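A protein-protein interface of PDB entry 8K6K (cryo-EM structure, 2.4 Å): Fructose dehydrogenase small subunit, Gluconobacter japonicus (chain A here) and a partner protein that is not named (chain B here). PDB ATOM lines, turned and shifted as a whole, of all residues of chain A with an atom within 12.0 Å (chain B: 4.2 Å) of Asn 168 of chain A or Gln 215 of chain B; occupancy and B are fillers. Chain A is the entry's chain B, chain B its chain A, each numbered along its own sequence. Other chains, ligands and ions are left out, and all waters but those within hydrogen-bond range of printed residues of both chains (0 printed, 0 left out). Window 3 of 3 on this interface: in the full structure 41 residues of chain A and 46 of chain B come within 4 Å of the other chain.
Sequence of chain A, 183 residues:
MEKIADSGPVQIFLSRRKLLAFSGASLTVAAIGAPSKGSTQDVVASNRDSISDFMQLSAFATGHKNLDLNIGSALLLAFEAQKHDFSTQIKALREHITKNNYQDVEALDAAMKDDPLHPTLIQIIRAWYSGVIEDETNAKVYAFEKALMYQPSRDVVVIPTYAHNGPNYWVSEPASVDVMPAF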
ATOM      1  N   ASP A 155     -22.645  35.039  19.899  1.00  0.00           N
ATOM      2  CA  ASP A 155     -23.877  34.308  20.159  1.00  0.00           C
ATOM      3  C   ASP A 155     -23.684  32.798  20.107  1.00  0.00           C
ATOM      4  O   ASP A 155     -24.551  32.062  20.584  1.00  0.00           O
ATOM      5  CB  ASP A 155     -24.956  34.730  19.164  1.00  0.00           C
ATOM      6  CG  ASP A 155     -24.570  34.447  17.732  1.00  0.00           C
ATOM      7  OD1 ASP A 155     -23.365  34.503  17.419  1.00  0.00           O
ATOM      8  OD2 ASP A 155     -25.471  34.169  16.916  1.00  0.00           O
ATOM      9  N   VAL A 156     -22.577  32.320  19.542  1.00  0.00           N
ATOM     10  CA  VAL A 156     -22.331  30.887  19.447  1.00  0.00           C
ATOM     11  C   VAL A 156     -21.026  30.528  20.141  1.00  0.00           C
ATOM     12  O   VAL A 156     -21.013  29.757  21.106  1.00  0.00           O
ATOM     13  CB  VAL A 156     -22.305  30.420  17.981  1.00  0.00           C
ATOM     14  CG1 VAL A 156     -22.198  28.913  17.921  1.00  0.00           C
ATOM     15  CG2 VAL A 156     -23.540  30.899  17.246  1.00  0.00           C
ATOM     16  N   VAL A 158     -17.658  30.694  22.327  1.00  0.00           N
ATOM     17  CA  VAL A 158     -17.265  31.244  23.616  1.00  0.00           C
ATOM     18  C   VAL A 158     -16.009  32.088  23.448  1.00  0.00           C
ATOM     19  O   VAL A 158     -15.097  31.734  22.694  1.00  0.00           O
ATOM     20  CB  VAL A 158     -17.043  30.107  24.630  1.00  0.00           C
ATOM     21  CG1 VAL A 158     -16.067  29.087  24.076  1.00  0.00           C
ATOM     22  CG2 VAL A 158     -16.541  30.648  25.951  1.00  0.00           C
ATOM     23  N   PRO A 160     -12.893  32.550  25.277  1.00  0.00           N
ATOM     24  CA  PRO A 160     -12.476  31.438  26.145  1.00  0.00           C
ATOM     25  C   PRO A 160     -12.546  31.655  27.652  1.00  0.00           C
ATOM     26  O   PRO A 160     -13.308  30.958  28.327  1.00  0.00           O
ATOM     27  CB  PRO A 160     -11.036  31.195  25.694  1.00  0.00           C
ATOM     28  CG  PRO A 160     -11.075  31.508  24.242  1.00  0.00           C
ATOM     29  CD  PRO A 160     -12.042  32.655  24.080  1.00  0.00           C
ATOM     30  N   THR A 161     -11.819  32.618  28.207  1.00  0.00           N
ATOM     31  CA  THR A 161     -11.784  32.655  29.666  1.00  0.00           C
ATOM     32  C   THR A 161     -13.067  33.193  30.290  1.00  0.00           C
ATOM     33  O   THR A 161     -13.114  33.344  31.514  1.00  0.00           O
ATOM     34  CB  THR A 161     -10.594  33.480  30.145  1.00  0.00           C
ATOM     35  OG1 THR A 161     -10.435  34.623  29.299  1.00  0.00           O
ATOM     36  CG2 THR A 161      -9.329  32.643  30.111  1.00  0.00           C
ATOM     37  N   TYR A 162     -14.097  33.478  29.501  1.00  0.00           N
ATOM     38  CA  TYR A 162     -15.374  33.961  30.004  1.00  0.00           C
ATOM     39  C   TYR A 162     -16.467  32.987  29.598  1.00  0.00           C
ATOM     40  O   TYR A 162     -16.602  32.658  28.417  1.00  0.00           O
ATOM     41  CB  TYR A 162     -15.674  35.362  29.478  1.00  0.00           C
ATOM     42  CG  TYR A 162     -14.698  36.398  29.973  1.00  0.00           C
ATOM     43  CD1 TYR A 162     -14.907  37.056  31.174  1.00  0.00           C
ATOM     44  CD2 TYR A 162     -13.562  36.711  29.245  1.00  0.00           C
ATOM     45  CE1 TYR A 162     -14.020  38.000  31.632  1.00  0.00           C
ATOM     46  CE2 TYR A 162     -12.667  37.654  29.695  1.00  0.00           C
ATOM     47  CZ  TYR A 162     -12.900  38.296  30.889  1.00  0.00           C
ATOM     48  OH  TYR A 162     -12.010  39.239  31.342  1.00  0.00           O
ATOM     49  N   ALA A 163     -17.247  32.539  30.574  1.00  0.00           N
ATOM     50  CA  ALA A 163     -18.185  31.450  30.356  1.00  0.00           C
ATOM     51  C   ALA A 163     -19.398  31.899  29.554  1.00  0.00           C
ATOM     52  O   ALA A 163     -19.891  33.018  29.713  1.00  0.00           O
ATOM     53  CB  ALA A 163     -18.641  30.874  31.694  1.00  0.00           C
ATOM     54  N   HIS A 164     -19.870  31.012  28.684  1.00  0.00           N
ATOM     55  CA  HIS A 164     -21.203  31.112  28.116  1.00  0.00           C
ATOM     56  C   HIS A 164     -22.220  30.651  29.160  1.00  0.00           C
ATOM     57  O   HIS A 164     -21.868  30.240  30.268  1.00  0.00           O
ATOM     58  CB  HIS A 164     -21.295  30.281  26.840  1.00  0.00           C
ATOM     59  CG  HIS A 164     -21.555  31.083  25.604  1.00  0.00           C
ATOM     60  ND1 HIS A 164     -22.651  30.867  24.796  1.00  0.00           N
ATOM     61  CD2 HIS A 164     -20.856  32.089  25.028  1.00  0.00           C
ATOM     62  CE1 HIS A 164     -22.619  31.710  23.780  1.00  0.00           C
ATOM     63  NE2 HIS A 164     -21.541  32.463  23.898  1.00  0.00           N
ATOM     64  N   ASN A 165     -23.502  30.693  28.809  1.00  0.00           N
ATOM     65  CA  ASN A 165     -24.530  30.475  29.819  1.00  0.00           C
ATOM     66  C   ASN A 165     -24.632  29.017  30.253  1.00  0.00           C
ATOM     67  O   ASN A 165     -25.358  28.230  29.641  1.00  0.00           O
ATOM     68  CB  ASN A 165     -25.889  30.963  29.312  1.00  0.00           C
ATOM     69  CG  ASN A 165     -26.230  30.424  27.944  1.00  0.00           C
ATOM     70  OD1 ASN A 165     -25.396  29.817  27.278  1.00  0.00           O
ATOM     71  ND2 ASN A 165     -27.468  30.634  27.519  1.00  0.00           N
ATOM     72  N   GLY A 166     -23.921  28.651  31.318  1.00  0.00           N
ATOM     73  CA  GLY A 166     -24.148  27.384  31.972  1.00  0.00           C
ATOM     74  C   GLY A 166     -23.135  26.309  31.639  1.00  0.00           C
ATOM     75  O   GLY A 166     -22.491  26.325  30.587  1.00  0.00           O
ATOM     76  N   PRO A 167     -22.984  25.340  32.547  1.00  0.00           N
ATOM     77  CA  PRO A 167     -21.978  24.288  32.359  1.00  0.00           C
ATOM     78  C   PRO A 167     -22.338  23.227  31.333  1.00  0.00           C
ATOM     79  O   PRO A 167     -21.572  22.270  31.181  1.00  0.00           O
ATOM     80  CB  PRO A 167     -21.864  23.665  33.759  1.00  0.00           C
ATOM     81  CG  PRO A 167     -22.383  24.696  34.677  1.00  0.00           C
ATOM     82  CD  PRO A 167     -23.486  25.364  33.926  1.00  0.00           C
ATOM     83  N   ASN A 168     -23.480  23.313  30.654  1.00  0.00           N
ATOM     84  CA  ASN A 168     -23.761  22.362  29.584  1.00  0.00           C
ATOM     85  C   ASN A 168     -24.484  23.021  28.418  1.00  0.00           C
ATOM     86  O   ASN A 168     -25.300  22.379  27.750  1.00  0.00           O
ATOM     87  CB  ASN A 168     -24.566  21.172  30.100  1.00  0.00           C
ATOM     88  CG  ASN A 168     -23.688  20.009  30.505  1.00  0.00           C
ATOM     89  OD1 ASN A 168     -22.687  19.720  29.855  1.00  0.00           O
ATOM     90  ND2 ASN A 168     -24.059  19.334  31.584  1.00  0.00           N
ATOM     91  N   TYR A 169     -24.200  24.298  28.158  1.00  0.00           N
ATOM     92  CA  TYR A 169     -24.926  25.034  27.130  1.00  0.00           C
ATOM     93  C   TYR A 169     -24.721  24.461  25.736  1.00  0.00           C
ATOM     94  O   TYR A 169     -25.572  24.667  24.865  1.00  0.00           O
ATOM     95  CB  TYR A 169     -24.505  26.505  27.145  1.00  0.00           C
ATOM     96  CG  TYR A 169     -23.121  26.753  26.591  1.00  0.00           C
ATOM     97  CD1 TYR A 169     -22.006  26.693  27.412  1.00  0.00           C
ATOM     98  CD2 TYR A 169     -22.928  27.048  25.249  1.00  0.00           C
ATOM     99  CE1 TYR A 169     -20.743  26.914  26.912  1.00  0.00           C
ATOM    100  CE2 TYR A 169     -21.670  27.268  24.742  1.00  0.00           C
ATOM    101  CZ  TYR A 169     -20.581  27.201  25.576  1.00  0.00           C
ATOM    102  OH  TYR A 169     -19.322  27.424  25.072  1.00  0.00           O
ATOM    103  N   TRP A 170     -23.622  23.747  25.501  1.00  0.00           N
ATOM    104  CA  TRP A 170     -23.259  23.357  24.144  1.00  0.00           C
ATOM    105  C   TRP A 170     -24.132  22.250  23.577  1.00  0.00           C
ATOM    106  O   TRP A 170     -23.980  21.923  22.396  1.00  0.00           O
ATOM    107  CB  TRP A 170     -21.792  22.936  24.091  1.00  0.00           C
ATOM    108  CG  TRP A 170     -21.373  22.011  25.180  1.00  0.00           C
ATOM    109  CD1 TRP A 170     -21.456  20.653  25.176  1.00  0.00           C
ATOM    110  CD2 TRP A 170     -20.784  22.372  26.429  1.00  0.00           C
ATOM    111  NE1 TRP A 170     -20.961  20.145  26.348  1.00  0.00           N
ATOM    112  CE2 TRP A 170     -20.540  21.182  27.135  1.00  0.00           C
ATOM    113  CE3 TRP A 170     -20.439  23.587  27.020  1.00  0.00           C
ATOM    114  CZ2 TRP A 170     -19.972  21.174  28.401  1.00  0.00           C
ATOM    115  CZ3 TRP A 170     -19.878  23.576  28.275  1.00  0.00           C
ATOM    116  CH2 TRP A 170     -19.644  22.379  28.949  1.00  0.00           C
ATOM    117  N   VAL A 171     -25.028  21.658  24.368  1.00  0.00           N
ATOM    118  CA  VAL A 171     -25.931  20.644  23.839  1.00  0.00           C
ATOM    119  C   VAL A 171     -26.953  21.215  22.871  1.00  0.00           C
ATOM    120  O   VAL A 171     -27.589  20.455  22.135  1.00  0.00           O
ATOM    121  CB  VAL A 171     -26.662  19.910  24.981  1.00  0.00           C
ATOM    122  CG1 VAL A 171     -25.673  19.473  26.035  1.00  0.00           C
ATOM    123  CG2 VAL A 171     -27.731  20.797  25.586  1.00  0.00           C
ATOM    124  N   SER A 172     -27.124  22.531  22.850  1.00  0.00           N
ATOM    125  CA  SER A 172     -28.078  23.175  21.963  1.00  0.00           C
ATOM    126  C   SER A 172     -27.477  23.366  20.575  1.00  0.00           C
ATOM    127  O   SER A 172     -26.261  23.434  20.399  1.00  0.00           O
ATOM    128  CB  SER A 172     -28.514  24.523  22.535  1.00  0.00           C
ATOM    129  OG  SER A 172     -27.434  25.437  22.553  1.00  0.00           O
ATOM    130  N   GLU A 173     -28.356  23.449  19.583  1.00  0.00           N
ATOM    131  CA  GLU A 173     -27.908  23.671  18.220  1.00  0.00           C
ATOM    132  C   GLU A 173     -27.434  25.113  18.053  1.00  0.00           C
ATOM    133  O   GLU A 173     -28.011  26.031  18.644  1.00  0.00           O
ATOM    134  CB  GLU A 173     -29.030  23.370  17.230  1.00  0.00           C
ATOM    135  CG  GLU A 173     -29.498  21.929  17.255  1.00  0.00           C
ATOM    136  CD  GLU A 173     -28.396  20.956  16.888  1.00  0.00           C
ATOM    137  OE1 GLU A 173     -27.766  21.146  15.827  1.00  0.00           O
ATOM    138  OE2 GLU A 173     -28.158  20.004  17.659  1.00  0.00           O
ATOM    139  N   PRO A 174     -26.394  25.346  17.261  1.00  0.00           N
ATOM    140  CA  PRO A 174     -25.899  26.708  17.062  1.00  0.00           C
ATOM    141  C   PRO A 174     -26.762  27.474  16.068  1.00  0.00           C
ATOM    142  O   PRO A 174     -27.561  26.910  15.321  1.00  0.00           O
ATOM    143  CB  PRO A 174     -24.484  26.494  16.517  1.00  0.00           C
ATOM    144  CG  PRO A 174     -24.505  25.144  15.898  1.00  0.00           C
ATOM    145  CD  PRO A 174     -25.656  24.359  16.457  1.00  0.00           C
ATOM    146  N   PRO B 179     -21.637  15.962  27.854  1.00  0.00           N
ATOM    147  CA  PRO B 179     -22.117  15.848  26.473  1.00  0.00           C
ATOM    148  C   PRO B 179     -21.252  16.626  25.494  1.00  0.00           C
ATOM    149  O   PRO B 179     -20.631  17.633  25.836  1.00  0.00           O
ATOM    150  CB  PRO B 179     -23.537  16.423  26.542  1.00  0.00           C
ATOM    151  CG  PRO B 179     -23.579  17.207  27.807  1.00  0.00           C
ATOM    152  CD  PRO B 179     -22.663  16.518  28.748  1.00  0.00           C
ATOM    153  N   ASN B 206     -14.495  18.178  35.405  1.00  0.00           N
ATOM    154  CA  ASN B 206     -15.694  18.032  36.225  1.00  0.00           C
ATOM    155  C   ASN B 206     -16.925  18.131  35.333  1.00  0.00           C
ATOM    156  O   ASN B 206     -17.306  19.221  34.903  1.00  0.00           O
ATOM    157  CB  ASN B 206     -15.721  19.088  37.323  1.00  0.00           C
ATOM    158  CG  ASN B 206     -14.722  18.810  38.419  1.00  0.00           C
ATOM    159  OD1 ASN B 206     -14.137  17.732  38.481  1.00  0.00           O
ATOM    160  ND2 ASN B 206     -14.519  19.783  39.293  1.00  0.00           N
ATOM    161  N   SER B 207     -17.550  16.988  35.055  1.00  0.00           N
ATOM    162  CA  SER B 207     -18.886  16.990  34.474  1.00  0.00           C
ATOM    163  C   SER B 207     -19.954  17.258  35.520  1.00  0.00           C
ATOM    164  O   SER B 207     -21.127  17.416  35.170  1.00  0.00           O
ATOM    165  CB  SER B 207     -19.167  15.661  33.778  1.00  0.00           C
ATOM    166  OG  SER B 207     -19.181  14.592  34.703  1.00  0.00           O
ATOM    167  N   ARG B 208     -19.563  17.300  36.787  1.00  0.00           N
ATOM    168  CA  ARG B 208     -20.402  17.682  37.909  1.00  0.00           C
ATOM    169  C   ARG B 208     -19.478  18.190  39.000  1.00  0.00           C
ATOM    170  O   ARG B 208     -18.273  17.922  38.963  1.00  0.00           O
ATOM    171  CB  ARG B 208     -21.242  16.500  38.408  1.00  0.00           C
ATOM    172  CG  ARG B 208     -20.422  15.334  38.915  1.00  0.00           C
ATOM    173  CD  ARG B 208     -21.305  14.230  39.455  1.00  0.00           C
ATOM    174  NE  ARG B 208     -20.535  13.041  39.797  1.00  0.00           N
ATOM    175  CZ  ARG B 208     -19.824  12.903  40.908  1.00  0.00           C
ATOM    176  NH1 ARG B 208     -19.766  13.864  41.814  1.00  0.00           N
ATOM    177  NH2 ARG B 208     -19.158  11.773  41.114  1.00  0.00           N
ATOM    178  N   PRO B 209     -19.995  18.950  39.962  1.00  0.00           N
ATOM    179  CA  PRO B 209     -19.145  19.401  41.068  1.00  0.00           C
ATOM    180  C   PRO B 209     -18.435  18.232  41.735  1.00  0.00           C
ATOM    181  O   PRO B 209     -19.063  17.277  42.197  1.00  0.00           O
ATOM    182  CB  PRO B 209     -20.137  20.079  42.013  1.00  0.00           C
ATOM    183  CG  PRO B 209     -21.190  20.584  41.115  1.00  0.00           C
ATOM    184  CD  PRO B 209     -21.328  19.574  40.013  1.00  0.00           C
ATOM    185  N   ARG B 213     -14.742  21.456  43.644  1.00  0.00           N
ATOM    186  CA  ARG B 213     -14.417  22.308  42.518  1.00  0.00           C
ATOM    187  C   ARG B 213     -15.600  22.378  41.561  1.00  0.00           C
ATOM    188  O   ARG B 213     -16.386  21.429  41.473  1.00  0.00           O
ATOM    189  CB  ARG B 213     -13.177  21.789  41.783  1.00  0.00           C
ATOM    190  CG  ARG B 213     -11.917  21.834  42.624  1.00  0.00           C
ATOM    191  CD  ARG B 213     -10.704  21.416  41.828  1.00  0.00           C
ATOM    192  NE  ARG B 213     -10.588  19.968  41.727  1.00  0.00           N
ATOM    193  CZ  ARG B 213     -10.792  19.276  40.616  1.00  0.00           C
ATOM    194  NH1 ARG B 213     -11.131  19.872  39.485  1.00  0.00           N
ATOM    195  NH2 ARG B 213     -10.652  17.955  40.639  1.00  0.00           N
ATOM    196  N   PRO B 214     -15.760  23.483  40.840  1.00  0.00           N
ATOM    197  CA  PRO B 214     -16.977  23.677  40.048  1.00  0.00           C
ATOM    198  C   PRO B 214     -17.042  22.747  38.849  1.00  0.00           C
ATOM    199  O   PRO B 214     -16.041  22.201  38.384  1.00  0.00           O
ATOM    200  CB  PRO B 214     -16.878  25.139  39.604  1.00  0.00           C
ATOM    201  CG  PRO B 214     -15.429  25.420  39.599  1.00  0.00           C
ATOM    202  CD  PRO B 214     -14.851  24.636  40.734  1.00  0.00           C
ATOM    203  N   GLN B 215     -18.263  22.563  38.358  1.00  0.00           N
ATOM    204  CA  GLN B 215     -18.479  21.844  37.114  1.00  0.00           C
ATOM    205  C   GLN B 215     -17.939  22.652  35.941  1.00  0.00           C
ATOM    206  O   GLN B 215     -17.969  23.885  35.943  1.00  0.00           O
ATOM    207  CB  GLN B 215     -19.969  21.560  36.920  1.00  0.00           C
ATOM    208  CG  GLN B 215     -20.299  20.726  35.702  1.00  0.00           C
ATOM    209  CD  GLN B 215     -21.784  20.505  35.540  1.00  0.00           C
ATOM    210  OE1 GLN B 215     -22.555  20.693  36.478  1.00  0.00           O
ATOM    211  NE2 GLN B 215     -22.197  20.103  34.346  1.00  0.00           N
ATOM    212  N   CYS B 216     -17.436  21.945  34.935  1.00  0.00           N
ATOM    213  CA  CYS B 216     -16.851  22.600  33.772  1.00  0.00           C
ATOM    214  C   CYS B 216     -17.920  23.367  33.006  1.00  0.00           C
ATOM    215  O   CYS B 216     -18.926  22.791  32.583  1.00  0.00           O
ATOM    216  CB  CYS B 216     -16.177  21.568  32.873  1.00  0.00           C
ATOM    217  SG  CYS B 216     -15.718  22.176  31.244  1.00  0.00           S
ATOM    218  N   CYS B 217     -17.695  24.665  32.821  1.00  0.00           N
ATOM    219  CA  CYS B 217     -18.620  25.529  32.102  1.00  0.00           C
ATOM    220  C   CYS B 217     -18.223  25.736  30.652  1.00  0.00           C
ATOM    221  O   CYS B 217     -18.762  26.631  29.997  1.00  0.00           O
ATOM    222  CB  CYS B 217     -18.735  26.883  32.801  1.00  0.00           C
ATOM    223  SG  CYS B 217     -17.188  27.788  32.957  1.00  0.00           S
ATOM    224  N   ILE B 228     -11.430  28.736  36.353  1.00  0.00           N
ATOM    225  CA  ILE B 228     -12.320  28.369  37.444  1.00  0.00           C
ATOM    226  C   ILE B 228     -11.899  27.091  38.147  1.00  0.00           C
ATOM    227  O   ILE B 228     -12.513  26.720  39.149  1.00  0.00           O
ATOM    228  CB  ILE B 228     -13.775  28.251  36.949  1.00  0.00           C
ATOM    229  CG1 ILE B 228     -13.973  26.952  36.175  1.00  0.00           C
ATOM    230  CG2 ILE B 228     -14.121  29.427  36.062  1.00  0.00           C
ATOM    231  CD1 ILE B 228     -15.421  26.605  35.944  1.00  0.00           C
ATOM    232  N   ALA B 230     -12.053  23.897  37.043  1.00  0.00           N
ATOM    233  CA  ALA B 230     -12.938  22.771  36.787  1.00  0.00           C
ATOM    234  C   ALA B 230     -12.208  21.577  36.193  1.00  0.00           C
ATOM    235  O   ALA B 230     -12.838  20.548  35.934  1.00  0.00           O
ATOM    236  CB  ALA B 230     -14.074  23.196  35.860  1.00  0.00           C
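The backbone carbonyl oxygen (O) of Asn 206 of chain B sits at hydrogen-bond distance from the backbone NH (N) of Cys 216 of chain B. O of Ser 207 of chain B is in hydrogen-bond range of NE2 of Gln 215 of chain B (3.0 Å). The backbone carbonyl oxygen (O) of Tyr 169 of chain A is in hydrogen-bond range of the side-chain hydroxyl (OG) of Ser 172 of chain A (3.1 Å).
The indole nitrogen (NE1) of Trp 170 of chain A is in hydrogen-bond range of the backbone carbonyl oxygen (O) of Pro 179 of chain B, at 2.6 Å. The side-chain amide nitrogen of Asn 168 of chain A lies close to the side-chain amide nitrogen of Gln 215 of chain B (3.4 Å). O of Pro 167 of chain A sits close to O of Cys 216 of chain B.
Of the 18 printed residues of chain A, 7 touch a printed residue of chain B. Printed residues of chain A that touch a printed residue of chain B: Ala 163, Gly 166, Pro 167, Asn 168, Tyr 169, Trp 170 and Val 171. Hydrophobic or aromatic side chains of chain A that line the printed part of chain B: Ala 163, Pro 167, Tyr 169, Trp 170 and Val 171. Among the printed residues, no Asp or Glu carboxylate lies within 4 Å of a Lys or Arg side-chain nitrogen of the other chain.
Among the printed residues, pairs that only touch across the chains: Asn 168 of chain A with Pro 179 of chain B, Val 171 of chain A with Pro 179 of chain B, Pro 167 of chain A with Cys 217 of chain B, Trp 170 of chain A with Cys 217 of chain B, Pro 167 of chain A with Gln 215 of chain B, Ala 163 of chain A with Cys 217 of chain B, Tyr 169 of chain A with Cys 217 of chain B, Trp 170 of chain A with Cys 216 of chain B and Gly 166 of chain A with Cys 217 of chain B.
Gln 215 of chain B touches two residues of chain A. Pro 179 of chain B touches just these residues of chain A: Asn 168, Trp 170 and Val 171. No residue of chain A comes within 4 Å of Asn 206 of chain B. Ser 207 of chain B touches none of the printed residues of chain A. No residue of chain A comes within 4 Å of Pro 209 of chain B. No residue of chain A comes within 4 Å of Pro 214 of chain B. Of the printed residues of chain B, Pro 167 of chain A touches Gln 215, Cys 216 and Cys 217. Printed residues of chain B within 4 Å of Trp 170 of chain A: Pro 179, Cys 216 and Cys 217. Of the printed residues of chain B, Tyr 169 of chain A touches Cys 217 (3.7 Å). Ile 228 of chain B touches none of the printed residues of chain A. The nearest printed residue of chain B that does not touch Pro 167 of chain A is Ser 207 of chain B (6.3 Å).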
